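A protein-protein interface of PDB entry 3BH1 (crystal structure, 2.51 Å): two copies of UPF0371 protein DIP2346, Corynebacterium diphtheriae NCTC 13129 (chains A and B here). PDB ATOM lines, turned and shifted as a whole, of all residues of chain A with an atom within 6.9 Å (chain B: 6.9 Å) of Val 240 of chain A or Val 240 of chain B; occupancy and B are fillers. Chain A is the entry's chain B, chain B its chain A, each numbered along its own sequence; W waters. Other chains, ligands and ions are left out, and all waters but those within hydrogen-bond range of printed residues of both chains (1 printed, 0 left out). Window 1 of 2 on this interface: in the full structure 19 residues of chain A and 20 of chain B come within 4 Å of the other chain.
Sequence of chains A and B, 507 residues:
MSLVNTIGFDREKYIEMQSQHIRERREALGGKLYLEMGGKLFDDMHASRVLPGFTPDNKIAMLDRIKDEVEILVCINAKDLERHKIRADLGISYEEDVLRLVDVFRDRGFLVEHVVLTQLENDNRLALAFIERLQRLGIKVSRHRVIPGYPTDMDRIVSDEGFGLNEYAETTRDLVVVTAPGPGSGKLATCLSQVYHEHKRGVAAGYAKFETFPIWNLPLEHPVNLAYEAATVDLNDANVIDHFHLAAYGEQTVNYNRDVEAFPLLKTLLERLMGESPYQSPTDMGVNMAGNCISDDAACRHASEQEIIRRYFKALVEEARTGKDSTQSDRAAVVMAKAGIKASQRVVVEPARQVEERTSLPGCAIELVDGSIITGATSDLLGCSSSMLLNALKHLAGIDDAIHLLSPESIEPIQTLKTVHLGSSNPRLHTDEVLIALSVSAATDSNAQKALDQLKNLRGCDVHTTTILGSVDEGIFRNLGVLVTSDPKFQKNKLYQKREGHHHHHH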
ATOM      1  N   PRO A 214      -2.478 -14.491  14.411  1.00  0.00           N
ATOM      2  CA  PRO A 214      -1.275 -15.332  14.452  1.00  0.00           C
ATOM      3  C   PRO A 214      -0.036 -14.536  14.050  1.00  0.00           C
ATOM      4  O   PRO A 214      -0.159 -13.420  13.535  1.00  0.00           O
ATOM      5  CB  PRO A 214      -1.574 -16.423  13.425  1.00  0.00           C
ATOM      6  CG  PRO A 214      -2.492 -15.794  12.467  1.00  0.00           C
ATOM      7  CD  PRO A 214      -3.307 -14.785  13.229  1.00  0.00           C
ATOM      8  N   LEU A 220       3.684 -22.135  10.917  1.00  0.00           N
ATOM      9  CA  LEU A 220       2.314 -22.565  11.209  1.00  0.00           C
ATOM     10  C   LEU A 220       2.299 -23.608  12.331  1.00  0.00           C
ATOM     11  O   LEU A 220       1.385 -23.632  13.157  1.00  0.00           O
ATOM     12  CB  LEU A 220       1.673 -23.137   9.941  1.00  0.00           C
ATOM     13  CG  LEU A 220       0.155 -23.061   9.764  1.00  0.00           C
ATOM     14  CD1 LEU A 220      -0.175 -22.918   8.291  1.00  0.00           C
ATOM     15  CD2 LEU A 220      -0.568 -24.273  10.368  1.00  0.00           C
ATOM     16  N   GLU A 229      -4.856 -20.923  17.711  1.00  0.00           N
ATOM     17  CA  GLU A 229      -5.900 -21.798  17.178  1.00  0.00           C
ATOM     18  C   GLU A 229      -6.718 -22.432  18.304  1.00  0.00           C
ATOM     19  O   GLU A 229      -7.934 -22.570  18.181  1.00  0.00           O
ATOM     20  CB  GLU A 229      -5.314 -22.885  16.272  1.00  0.00           C
ATOM     21  CG  GLU A 229      -4.759 -22.378  14.956  1.00  0.00           C
ATOM     22  CD  GLU A 229      -4.540 -23.486  13.936  1.00  0.00           C
ATOM     23  OE1 GLU A 229      -3.797 -24.446  14.232  1.00  0.00           O
ATOM     24  OE2 GLU A 229      -5.103 -23.391  12.825  1.00  0.00           O
ATOM     25  N   LEU A 235     -13.600 -21.978  12.228  1.00  0.00           N
ATOM     26  CA  LEU A 235     -12.658 -22.274  11.141  1.00  0.00           C
ATOM     27  C   LEU A 235     -12.166 -21.000  10.418  1.00  0.00           C
ATOM     28  O   LEU A 235     -11.084 -20.995   9.831  1.00  0.00           O
ATOM     29  CB  LEU A 235     -13.290 -23.275  10.158  1.00  0.00           C
ATOM     30  CG  LEU A 235     -12.627 -23.624   8.815  1.00  0.00           C
ATOM     31  CD1 LEU A 235     -11.361 -24.461   9.002  1.00  0.00           C
ATOM     32  CD2 LEU A 235     -13.614 -24.331   7.904  1.00  0.00           C
ATOM     33  N   ASP A 237     -10.924 -18.515  11.831  1.00  0.00           N
ATOM     34  CA  ASP A 237      -9.729 -18.082  12.539  1.00  0.00           C
ATOM     35  C   ASP A 237      -8.555 -19.053  12.378  1.00  0.00           C
ATOM     36  O   ASP A 237      -7.469 -18.793  12.891  1.00  0.00           O
ATOM     37  CB  ASP A 237     -10.047 -17.863  14.020  1.00  0.00           C
ATOM     38  CG  ASP A 237     -11.320 -17.042  14.236  1.00  0.00           C
ATOM     39  OD1 ASP A 237     -11.459 -15.963  13.616  1.00  0.00           O
ATOM     40  OD2 ASP A 237     -12.184 -17.481  15.027  1.00  0.00           O
ATOM     41  N   ALA A 238      -8.776 -20.153  11.658  1.00  0.00           N
ATOM     42  CA  ALA A 238      -7.749 -21.178  11.468  1.00  0.00           C
ATOM     43  C   ALA A 238      -6.598 -20.695  10.585  1.00  0.00           C
ATOM     44  O   ALA A 238      -6.815 -20.119   9.519  1.00  0.00           O
ATOM     45  CB  ALA A 238      -8.356 -22.457  10.906  1.00  0.00           C
ATOM     46  N   ASN A 239      -5.381 -20.924  11.063  1.00  0.00           N
ATOM     47  CA  ASN A 239      -4.168 -20.528  10.369  1.00  0.00           C
ATOM     48  C   ASN A 239      -3.962 -21.243   9.041  1.00  0.00           C
ATOM     49  O   ASN A 239      -4.201 -22.441   8.919  1.00  0.00           O
ATOM     50  CB  ASN A 239      -2.952 -20.745  11.269  1.00  0.00           C
ATOM     51  CG  ASN A 239      -2.966 -19.851  12.491  1.00  0.00           C
ATOM     52  OD1 ASN A 239      -3.801 -18.950  12.621  1.00  0.00           O
ATOM     53  ND2 ASN A 239      -2.036 -20.099  13.400  1.00  0.00           N
ATOM     54  N   VAL A 240      -3.544 -20.482   8.041  1.00  0.00           N
ATOM     55  CA  VAL A 240      -3.229 -21.023   6.731  1.00  0.00           C
ATOM     56  C   VAL A 240      -1.942 -20.364   6.248  1.00  0.00           C
ATOM     57  O   VAL A 240      -1.543 -19.307   6.752  1.00  0.00           O
ATOM     58  CB  VAL A 240      -4.368 -20.774   5.684  1.00  0.00           C
ATOM     59  CG1 VAL A 240      -5.623 -21.573   6.011  1.00  0.00           C
ATOM     60  CG2 VAL A 240      -4.699 -19.291   5.567  1.00  0.00           C
ATOM     61  N   ILE A 241      -1.295 -20.996   5.279  1.00  0.00           N
ATOM     62  CA  ILE A 241      -0.169 -20.395   4.586  1.00  0.00           C
ATOM     63  C   ILE A 241      -0.688 -19.291   3.674  1.00  0.00           C
ATOM     64  O   ILE A 241      -1.585 -19.529   2.866  1.00  0.00           O
ATOM     65  CB  ILE A 241       0.605 -21.459   3.795  1.00  0.00           C
ATOM     66  CG1 ILE A 241       1.269 -22.416   4.788  1.00  0.00           C
ATOM     67  CG2 ILE A 241       1.612 -20.811   2.842  1.00  0.00           C
ATOM     68  CD1 ILE A 241       2.381 -23.219   4.243  1.00  0.00           C
ATOM     69  N   ASP A 242      -0.154 -18.083   3.853  1.00  0.00           N
ATOM     70  CA  ASP A 242      -0.513 -16.915   3.045  1.00  0.00           C
ATOM     71  C   ASP A 242      -0.025 -17.141   1.621  1.00  0.00           C
ATOM     72  O   ASP A 242       1.102 -16.770   1.270  1.00  0.00           O
ATOM     73  CB  ASP A 242       0.110 -15.639   3.644  1.00  0.00           C
ATOM     74  CG  ASP A 242      -0.311 -14.357   2.915  1.00  0.00           C
ATOM     75  OD1 ASP A 242      -0.831 -14.410   1.780  1.00  0.00           O
ATOM     76  OD2 ASP A 242      -0.105 -13.266   3.484  1.00  0.00           O
ATOM     77  N   HIS A 243      -0.896 -17.728   0.806  1.00  0.00           N
ATOM     78  CA  HIS A 243      -0.554 -18.100  -0.560  1.00  0.00           C
ATOM     79  C   HIS A 243      -0.346 -16.912  -1.489  1.00  0.00           C
ATOM     80  O   HIS A 243       0.310 -17.044  -2.525  1.00  0.00           O
ATOM     81  CB  HIS A 243      -1.568 -19.101  -1.131  1.00  0.00           C
ATOM     82  CG  HIS A 243      -2.944 -18.550  -1.329  1.00  0.00           C
ATOM     83  ND1 HIS A 243      -3.261 -17.685  -2.352  1.00  0.00           N
ATOM     84  CD2 HIS A 243      -4.097 -18.779  -0.660  1.00  0.00           C
ATOM     85  CE1 HIS A 243      -4.545 -17.384  -2.293  1.00  0.00           C
ATOM     86  NE2 HIS A 243      -5.076 -18.033  -1.273  1.00  0.00           N
ATOM     87  N   THR A 253       4.693 -17.538   4.940  1.00  0.00           N
ATOM     88  CA  THR A 253       4.198 -16.773   6.082  1.00  0.00           C
ATOM     89  C   THR A 253       2.802 -17.243   6.491  1.00  0.00           C
ATOM     90  O   THR A 253       2.129 -17.955   5.745  1.00  0.00           O
ATOM     91  CB  THR A 253       4.139 -15.248   5.795  1.00  0.00           C
ATOM     92  OG1 THR A 253       3.360 -15.005   4.619  1.00  0.00           O
ATOM     93  CG2 THR A 253       5.525 -14.657   5.608  1.00  0.00           C
ATOM     94  N   VAL A 254       2.365 -16.812   7.671  1.00  0.00           N
ATOM     95  CA  VAL A 254       1.141 -17.312   8.274  1.00  0.00           C
ATOM     96  C   VAL A 254       0.092 -16.222   8.353  1.00  0.00           C
ATOM     97  O   VAL A 254       0.337 -15.139   8.891  1.00  0.00           O
ATOM     98  CB  VAL A 254       1.407 -17.899   9.689  1.00  0.00           C
ATOM     99  CG1 VAL A 254       0.092 -18.252  10.419  1.00  0.00           C
ATOM    100  CG2 VAL A 254       2.289 -19.113   9.579  1.00  0.00           C
ATOM    101  N   ASN A 255      -1.070 -16.514   7.784  1.00  0.00           N
ATOM    102  CA  ASN A 255      -2.259 -15.711   7.999  1.00  0.00           C
ATOM    103  C   ASN A 255      -3.373 -16.682   8.383  1.00  0.00           C
ATOM    104  O   ASN A 255      -3.096 -17.764   8.903  1.00  0.00           O
ATOM    105  CB  ASN A 255      -2.585 -14.906   6.736  1.00  0.00           C
ATOM    106  CG  ASN A 255      -3.534 -13.745   7.005  1.00  0.00           C
ATOM    107  OD1 ASN A 255      -4.751 -13.894   6.896  1.00  0.00           O
ATOM    108  ND2 ASN A 255      -2.985 -12.588   7.349  1.00  0.00           N
ATOM    109  N   TYR A 256      -4.621 -16.323   8.115  1.00  0.00           N
ATOM    110  CA  TYR A 256      -5.753 -17.133   8.523  1.00  0.00           C
ATOM    111  C   TYR A 256      -6.905 -17.007   7.542  1.00  0.00           C
ATOM    112  O   TYR A 256      -6.957 -16.057   6.756  1.00  0.00           O
ATOM    113  CB  TYR A 256      -6.183 -16.807   9.962  1.00  0.00           C
ATOM    114  CG  TYR A 256      -6.557 -15.363  10.242  1.00  0.00           C
ATOM    115  CD1 TYR A 256      -5.574 -14.375  10.379  1.00  0.00           C
ATOM    116  CD2 TYR A 256      -7.893 -14.990  10.418  1.00  0.00           C
ATOM    117  CE1 TYR A 256      -5.907 -13.058  10.651  1.00  0.00           C
ATOM    118  CE2 TYR A 256      -8.241 -13.662  10.691  1.00  0.00           C
ATOM    119  CZ  TYR A 256      -7.243 -12.709  10.809  1.00  0.00           C
ATOM    120  OH  TYR A 256      -7.570 -11.406  11.085  1.00  0.00           O
ATOM    121  N   ASN A 257      -7.814 -17.980   7.597  1.00  0.00           N
ATOM    122  CA  ASN A 257      -8.913 -18.104   6.640  1.00  0.00           C
ATOM    123  C   ASN A 257      -9.707 -16.837   6.319  1.00  0.00           C
ATOM    124  O   ASN A 257      -9.841 -16.499   5.148  1.00  0.00           O
ATOM    125  CB  ASN A 257      -9.852 -19.248   7.038  1.00  0.00           C
ATOM    126  CG  ASN A 257      -9.459 -20.570   6.405  1.00  0.00           C
ATOM    127  OD1 ASN A 257      -9.221 -20.645   5.200  1.00  0.00           O
ATOM    128  ND2 ASN A 257      -9.396 -21.622   7.211  1.00  0.00           N
ATOM    129  N   ARG A 258     -10.199 -16.129   7.336  1.00  0.00           N
ATOM    130  CA  ARG A 258     -11.046 -14.956   7.102  1.00  0.00           C
ATOM    131  C   ARG A 258     -10.352 -13.857   6.288  1.00  0.00           C
ATOM    132  O   ARG A 258     -10.906 -13.383   5.301  1.00  0.00           O
ATOM    133  CB  ARG A 258     -11.610 -14.386   8.412  1.00  0.00           C
ATOM    134  CG  ARG A 258     -12.631 -13.270   8.199  1.00  0.00           C
ATOM    135  CD  ARG A 258     -13.007 -12.549   9.482  1.00  0.00           C
ATOM    136  NE  ARG A 258     -13.906 -13.351  10.310  1.00  0.00           N
ATOM    137  CZ  ARG A 258     -13.540 -14.003  11.413  1.00  0.00           C
ATOM    138  NH1 ARG A 258     -14.439 -14.710  12.091  1.00  0.00           N
ATOM    139  NH2 ARG A 258     -12.282 -13.950  11.843  1.00  0.00           N
ATOM    140  N   VAL A 260      -7.570 -14.129   4.453  1.00  0.00           N
ATOM    141  CA  VAL A 260      -7.091 -14.641   3.168  1.00  0.00           C
ATOM    142  C   VAL A 260      -8.248 -14.684   2.172  1.00  0.00           C
ATOM    143  O   VAL A 260      -8.096 -14.312   1.001  1.00  0.00           O
ATOM    144  CB  VAL A 260      -6.403 -16.021   3.331  1.00  0.00           C
ATOM    145  CG1 VAL A 260      -6.269 -16.743   2.004  1.00  0.00           C
ATOM    146  CG2 VAL A 260      -5.039 -15.849   3.969  1.00  0.00           C
ATOM    147  N   PRO B 214     -10.001 -30.294  -5.512  1.00  0.00           N
ATOM    148  CA  PRO B 214      -9.072 -29.507  -6.330  1.00  0.00           C
ATOM    149  C   PRO B 214      -7.915 -30.360  -6.847  1.00  0.00           C
ATOM    150  O   PRO B 214      -7.678 -31.448  -6.336  1.00  0.00           O
ATOM    151  CB  PRO B 214      -8.545 -28.462  -5.350  1.00  0.00           C
ATOM    152  CG  PRO B 214      -8.659 -29.100  -4.028  1.00  0.00           C
ATOM    153  CD  PRO B 214      -9.913 -29.918  -4.091  1.00  0.00           C
ATOM    154  N   LEU B 220      -2.792 -23.002  -6.944  1.00  0.00           N
ATOM    155  CA  LEU B 220      -3.999 -22.508  -6.272  1.00  0.00           C
ATOM    156  C   LEU B 220      -4.677 -21.396  -7.082  1.00  0.00           C
ATOM    157  O   LEU B 220      -5.887 -21.204  -6.998  1.00  0.00           O
ATOM    158  CB  LEU B 220      -3.623 -21.982  -4.889  1.00  0.00           C
ATOM    159  CG  LEU B 220      -4.498 -22.239  -3.666  1.00  0.00           C
ATOM    160  CD1 LEU B 220      -3.630 -22.094  -2.446  1.00  0.00           C
ATOM    161  CD2 LEU B 220      -5.686 -21.288  -3.578  1.00  0.00           C
ATOM    162  N   GLU B 229     -13.610 -23.780  -6.522  1.00  0.00           N
ATOM    163  CA  GLU B 229     -13.969 -22.880  -5.419  1.00  0.00           C
ATOM    164  C   GLU B 229     -15.286 -22.163  -5.684  1.00  0.00           C
ATOM    165  O   GLU B 229     -16.116 -22.028  -4.782  1.00  0.00           O
ATOM    166  CB  GLU B 229     -12.855 -21.878  -5.116  1.00  0.00           C
ATOM    167  CG  GLU B 229     -11.697 -22.479  -4.349  1.00  0.00           C
ATOM    168  CD  GLU B 229     -10.783 -21.432  -3.738  1.00  0.00           C
ATOM    169  OE1 GLU B 229     -10.133 -20.686  -4.498  1.00  0.00           O
ATOM    170  OE2 GLU B 229     -10.697 -21.367  -2.494  1.00  0.00           O
ATOM    171  N   LEU B 235     -16.794 -22.675   3.504  1.00  0.00           N
ATOM    172  CA  LEU B 235     -15.386 -22.374   3.790  1.00  0.00           C
ATOM    173  C   LEU B 235     -14.551 -23.652   3.925  1.00  0.00           C
ATOM    174  O   LEU B 235     -13.378 -23.675   3.551  1.00  0.00           O
ATOM    175  CB  LEU B 235     -15.260 -21.507   5.048  1.00  0.00           C
ATOM    176  CG  LEU B 235     -13.866 -21.071   5.520  1.00  0.00           C
ATOM    177  CD1 LEU B 235     -13.114 -20.263   4.453  1.00  0.00           C
ATOM    178  CD2 LEU B 235     -13.992 -20.283   6.803  1.00  0.00           C
ATOM    179  N   ASP B 237     -14.573 -26.171   2.123  1.00  0.00           N
ATOM    180  CA  ASP B 237     -14.190 -26.704   0.821  1.00  0.00           C
ATOM    181  C   ASP B 237     -13.216 -25.785   0.081  1.00  0.00           C
ATOM    182  O   ASP B 237     -12.765 -26.118  -1.022  1.00  0.00           O
ATOM    183  CB  ASP B 237     -15.430 -26.977  -0.047  1.00  0.00           C
ATOM    184  CG  ASP B 237     -16.460 -27.876   0.636  1.00  0.00           C
ATOM    185  OD1 ASP B 237     -16.087 -28.927   1.215  1.00  0.00           O
ATOM    186  OD2 ASP B 237     -17.661 -27.529   0.574  1.00  0.00           O
ATOM    187  N   ALA B 238     -12.891 -24.643   0.688  1.00  0.00           N
ATOM    188  CA  ALA B 238     -11.974 -23.667   0.086  1.00  0.00           C
ATOM    189  C   ALA B 238     -10.539 -24.178   0.012  1.00  0.00           C
ATOM    190  O   ALA B 238     -10.035 -24.800   0.951  1.00  0.00           O
ATOM    191  CB  ALA B 238     -12.020 -22.357   0.832  1.00  0.00           C
ATOM    192  N   ASN B 239      -9.898 -23.909  -1.120  1.00  0.00           N
ATOM    193  CA  ASN B 239      -8.522 -24.326  -1.370  1.00  0.00           C
ATOM    194  C   ASN B 239      -7.501 -23.661  -0.437  1.00  0.00           C
ATOM    195  O   ASN B 239      -7.499 -22.437  -0.257  1.00  0.00           O
ATOM    196  CB  ASN B 239      -8.153 -24.081  -2.841  1.00  0.00           C
ATOM    197  CG  ASN B 239      -8.896 -24.995  -3.793  1.00  0.00           C
ATOM    198  OD1 ASN B 239      -9.549 -25.948  -3.374  1.00  0.00           O
ATOM    199  ND2 ASN B 239      -8.790 -24.715  -5.087  1.00  0.00           N
ATOM    200  N   VAL B 240      -6.669 -24.487   0.188  1.00  0.00           N
ATOM    201  CA  VAL B 240      -5.536 -24.010   0.979  1.00  0.00           C
ATOM    202  C   VAL B 240      -4.276 -24.724   0.492  1.00  0.00           C
ATOM    203  O   VAL B 240      -4.362 -25.825  -0.065  1.00  0.00           O
ATOM    204  CB  VAL B 240      -5.725 -24.243   2.519  1.00  0.00           C
ATOM    205  CG1 VAL B 240      -6.994 -23.579   3.034  1.00  0.00           C
ATOM    206  CG2 VAL B 240      -5.728 -25.744   2.891  1.00  0.00           C
ATOM    207  N   ILE B 241      -3.114 -24.105   0.684  1.00  0.00           N
ATOM    208  CA  ILE B 241      -1.847 -24.831   0.536  1.00  0.00           C
ATOM    209  C   ILE B 241      -1.716 -25.934   1.601  1.00  0.00           C
ATOM    210  O   ILE B 241      -1.925 -25.686   2.793  1.00  0.00           O
ATOM    211  CB  ILE B 241      -0.639 -23.873   0.559  1.00  0.00           C
ATOM    212  CG1 ILE B 241      -0.487 -23.228  -0.819  1.00  0.00           C
ATOM    213  CG2 ILE B 241       0.651 -24.607   0.939  1.00  0.00           C
ATOM    214  CD1 ILE B 241       0.451 -22.093  -0.856  1.00  0.00           C
ATOM    215  N   ASP B 242      -1.420 -27.153   1.144  1.00  0.00           N
ATOM    216  CA  ASP B 242      -1.165 -28.297   2.016  1.00  0.00           C
ATOM    217  C   ASP B 242       0.124 -28.053   2.783  1.00  0.00           C
ATOM    218  O   ASP B 242       1.217 -28.329   2.270  1.00  0.00           O
ATOM    219  CB  ASP B 242      -1.029 -29.567   1.168  1.00  0.00           C
ATOM    220  CG  ASP B 242      -0.906 -30.844   2.000  1.00  0.00           C
ATOM    221  OD1 ASP B 242      -0.474 -30.815   3.177  1.00  0.00           O
ATOM    222  OD2 ASP B 242      -1.231 -31.912   1.448  1.00  0.00           O
ATOM    223  N   HIS B 243      -0.006 -27.559   4.014  1.00  0.00           N
ATOM    224  CA  HIS B 243       1.170 -27.210   4.810  1.00  0.00           C
ATOM    225  C   HIS B 243       1.939 -28.407   5.357  1.00  0.00           C
ATOM    226  O   HIS B 243       3.133 -28.296   5.633  1.00  0.00           O
ATOM    227  CB  HIS B 243       0.855 -26.189   5.914  1.00  0.00           C
ATOM    228  CG  HIS B 243      -0.135 -26.657   6.930  1.00  0.00           C
ATOM    229  ND1 HIS B 243       0.216 -27.451   8.000  1.00  0.00           N
ATOM    230  CD2 HIS B 243      -1.456 -26.405   7.066  1.00  0.00           C
ATOM    231  CE1 HIS B 243      -0.852 -27.686   8.739  1.00  0.00           C
ATOM    232  NE2 HIS B 243      -1.880 -27.064   8.194  1.00  0.00           N
ATOM    233  N   THR B 253       1.677 -27.824  -2.851  1.00  0.00           N
ATOM    234  CA  THR B 253       0.530 -28.540  -3.419  1.00  0.00           C
ATOM    235  C   THR B 253      -0.786 -28.021  -2.839  1.00  0.00           C
ATOM    236  O   THR B 253      -0.814 -27.432  -1.753  1.00  0.00           O
ATOM    237  CB  THR B 253       0.615 -30.069  -3.174  1.00  0.00           C
ATOM    238  OG1 THR B 253       0.658 -30.332  -1.766  1.00  0.00           O
ATOM    239  CG2 THR B 253       1.851 -30.675  -3.849  1.00  0.00           C
ATOM    240  N   VAL B 254      -1.876 -28.257  -3.561  1.00  0.00           N
ATOM    241  CA  VAL B 254      -3.181 -27.743  -3.179  1.00  0.00           C
ATOM    242  C   VAL B 254      -4.020 -28.822  -2.511  1.00  0.00           C
ATOM    243  O   VAL B 254      -4.124 -29.947  -3.002  1.00  0.00           O
ATOM    244  CB  VAL B 254      -3.939 -27.152  -4.395  1.00  0.00           C
ATOM    245  CG1 VAL B 254      -5.373 -26.713  -4.015  1.00  0.00           C
ATOM    246  CG2 VAL B 254      -3.182 -25.983  -4.943  1.00  0.00           C
ATOM    247  N   ASN B 255      -4.592 -28.464  -1.372  1.00  0.00           N
ATOM    248  CA  ASN B 255      -5.624 -29.255  -0.733  1.00  0.00           C
ATOM    249  C   ASN B 255      -6.695 -28.255  -0.262  1.00  0.00           C
ATOM    250  O   ASN B 255      -6.792 -27.161  -0.803  1.00  0.00           O
ATOM    251  CB  ASN B 255      -5.022 -30.093   0.403  1.00  0.00           C
ATOM    252  CG  ASN B 255      -5.833 -31.341   0.716  1.00  0.00           C
ATOM    253  OD1 ASN B 255      -5.535 -32.430   0.228  1.00  0.00           O
ATOM    254  ND2 ASN B 255      -6.849 -31.191   1.547  1.00  0.00           N
ATOM    255  N   TYR B 256      -7.493 -28.613   0.728  1.00  0.00           N
ATOM    256  CA  TYR B 256      -8.580 -27.761   1.172  1.00  0.00           C
ATOM    257  C   TYR B 256      -8.831 -27.924   2.660  1.00  0.00           C
ATOM    258  O   TYR B 256      -8.401 -28.915   3.264  1.00  0.00           O
ATOM    259  CB  TYR B 256      -9.853 -28.028   0.359  1.00  0.00           C
ATOM    260  CG  TYR B 256     -10.375 -29.451   0.388  1.00  0.00           C
ATOM    261  CD1 TYR B 256      -9.871 -30.418  -0.481  1.00  0.00           C
ATOM    262  CD2 TYR B 256     -11.398 -29.823   1.262  1.00  0.00           C
ATOM    263  CE1 TYR B 256     -10.352 -31.716  -0.468  1.00  0.00           C
ATOM    264  CE2 TYR B 256     -11.888 -31.127   1.283  1.00  0.00           C
ATOM    265  CZ  TYR B 256     -11.358 -32.062   0.410  1.00  0.00           C
ATOM    266  OH  TYR B 256     -11.834 -33.349   0.408  1.00  0.00           O
ATOM    267  N   ASN B 257      -9.535 -26.948   3.231  1.00  0.00           N
ATOM    268  CA  ASN B 257      -9.746 -26.845   4.674  1.00  0.00           C
ATOM    269  C   ASN B 257     -10.183 -28.126   5.394  1.00  0.00           C
ATOM    270  O   ASN B 257      -9.533 -28.526   6.354  1.00  0.00           O
ATOM    271  CB  ASN B 257     -10.718 -25.700   4.993  1.00  0.00           C
ATOM    272  CG  ASN B 257     -10.027 -24.346   5.088  1.00  0.00           C
ATOM    273  OD1 ASN B 257      -8.982 -24.203   5.728  1.00  0.00           O
ATOM    274  ND2 ASN B 257     -10.628 -23.339   4.470  1.00  0.00           N
ATOM    275  N   ARG B 258     -11.259 -28.768   4.928  1.00  0.00           N
ATOM    276  CA  ARG B 258     -11.826 -29.926   5.636  1.00  0.00           C
ATOM    277  C   ARG B 258     -10.822 -31.060   5.824  1.00  0.00           C
ATOM    278  O   ARG B 258     -10.646 -31.556   6.941  1.00  0.00           O
ATOM    279  CB  ARG B 258     -13.097 -30.446   4.956  1.00  0.00           C
ATOM    280  CG  ARG B 258     -13.647 -31.721   5.589  1.00  0.00           C
ATOM    281  CD  ARG B 258     -15.047 -32.047   5.125  1.00  0.00           C
ATOM    282  NE  ARG B 258     -16.054 -31.250   5.825  1.00  0.00           N
ATOM    283  CZ  ARG B 258     -16.859 -30.369   5.236  1.00  0.00           C
ATOM    284  NH1 ARG B 258     -17.744 -29.699   5.964  1.00  0.00           N
ATOM    285  NH2 ARG B 258     -16.785 -30.158   3.922  1.00  0.00           N
ATOM    286  N   VAL B 260      -7.494 -30.857   5.431  1.00  0.00           N
ATOM    287  CA  VAL B 260      -6.305 -30.369   6.142  1.00  0.00           C
ATOM    288  C   VAL B 260      -6.512 -30.343   7.667  1.00  0.00           C
ATOM    289  O   VAL B 260      -5.621 -30.724   8.430  1.00  0.00           O
ATOM    290  CB  VAL B 260      -5.796 -29.018   5.563  1.00  0.00           C
ATOM    291  CG1 VAL B 260      -4.739 -28.379   6.462  1.00  0.00           C
ATOM    292  CG2 VAL B 260      -5.196 -29.249   4.173  1.00  0.00           C
HETATM  293  O   HOH W   1      -3.346 -21.633   1.969  1.00  0.00           O
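OD1 of Asn 257 of chain B is in hydrogen-bond range of ND2 of Asn 257 of chain A, 3.0 Å away.
Hydrophobic or aromatic side chains of chain B that line the printed part of chain A: Leu 220, Leu 235, Val 240, Ile 241 and His 243.
Hydrophobic or aromatic side chains of chain A within 4 Å of the printed part of chain B: Leu 220, Val 240, Ile 241 and His 243.
Among the printed residues, 8 pairs touch across the chains.
Val 240 of chain A touches just one residue of chain B: Val 240.
Of the printed residues of chain B, Asn 257 of chain A touches Leu 235 (3.98 Å) and Asn 257 (3.0 Å).
Of the printed residues of chain A, Leu 235 of chain B touches Asn 257.
Printed residues of chain A within 4 Å of His 243 of chain B: Leu 220 and Ile 241.
Arg 258 of chain B touches none of the printed residues of chain A.
The nearest printed residue of chain A that does not touch Leu 220 of chain B is Ile 241 of chain A (6.2 Å).
Leu 220 of chain A touches His 243 of chain B (CD2 to NE2, 3.8 Å).
Val 240 of chain B touches Val 240 of chain A.
Ile 241 of chain A touches Ile 241 of chain B (CD1 to CG2, 3.98 Å).
Ile 241 of chain A touches His 243 of chain B (CD1 to CB, 3.7 Å).
Leu 220 of chain B touches His 243 of chain A (CD1 to CG, 3.8 Å).
Ile 241 of chain B touches His 243 of chain A (CD1 to CB, 3.6 Å).
OD1 of Asn 257 of chain A touches CD1 of Leu 235 of chain B, 3.98 Å away.
Leu 220 of chain A touches His 243 of chain B, and with the chains exchanged His 243 of chain A touches Leu 220 of chain B.
Val 240 of chain A touches its own counterpart, Val 240 of chain B.
Ile 241 of chain A touches His 243 of chain B, and with the chains exchanged His 243 of chain A touches Ile 241 of chain B.
Asn 257 of chain A touches Leu 235 of chain B, but with the chains exchanged Leu 235 of chain A does not touch Asn 257 of chain B (4.1 Å).
Positions printed for both chains: 214, 220, 229, 235, 237, 238, 239, 240, 241, 242, 243, 253, 254, 255, 256, 257, 258 and 260.
Of the 8 pairs that touch across the chains among the printed residues, 7 have their exchanged pair printed and touching as well.
Water W1 bridges N of Ile 241 of chain B and O of Ile 241 of chain A.
The backbone carbonyl oxygen (O) of Leu 235 of chain B is in hydrogen-bond range of the side-chain amide nitrogen (ND2) of Asn 257 of chain B.
The backbone carbonyl oxygen of Ala 238 of chain B sits at hydrogen-bond distance from the backbone NH of Asn 257 of chain B, at 3.2 Å.
The backbone NH of Val 240 of chain B is in hydrogen-bond range of the backbone carbonyl oxygen of Asn 255 of chain B (2.9 Å).
O of Leu 235 of chain A is in hydrogen-bond range of ND2 of Asn 257 of chain A, at 3.2 Å.
The backbone NH (N) of Asn 257 of chain A lies within hydrogen-bond range of the backbone carbonyl oxygen (O) of Ala 238 of chain A.
The backbone NH (N) of Val 240 of chain A sits at hydrogen-bond distance from the backbone carbonyl oxygen (O) of Asn 255 of chain A.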
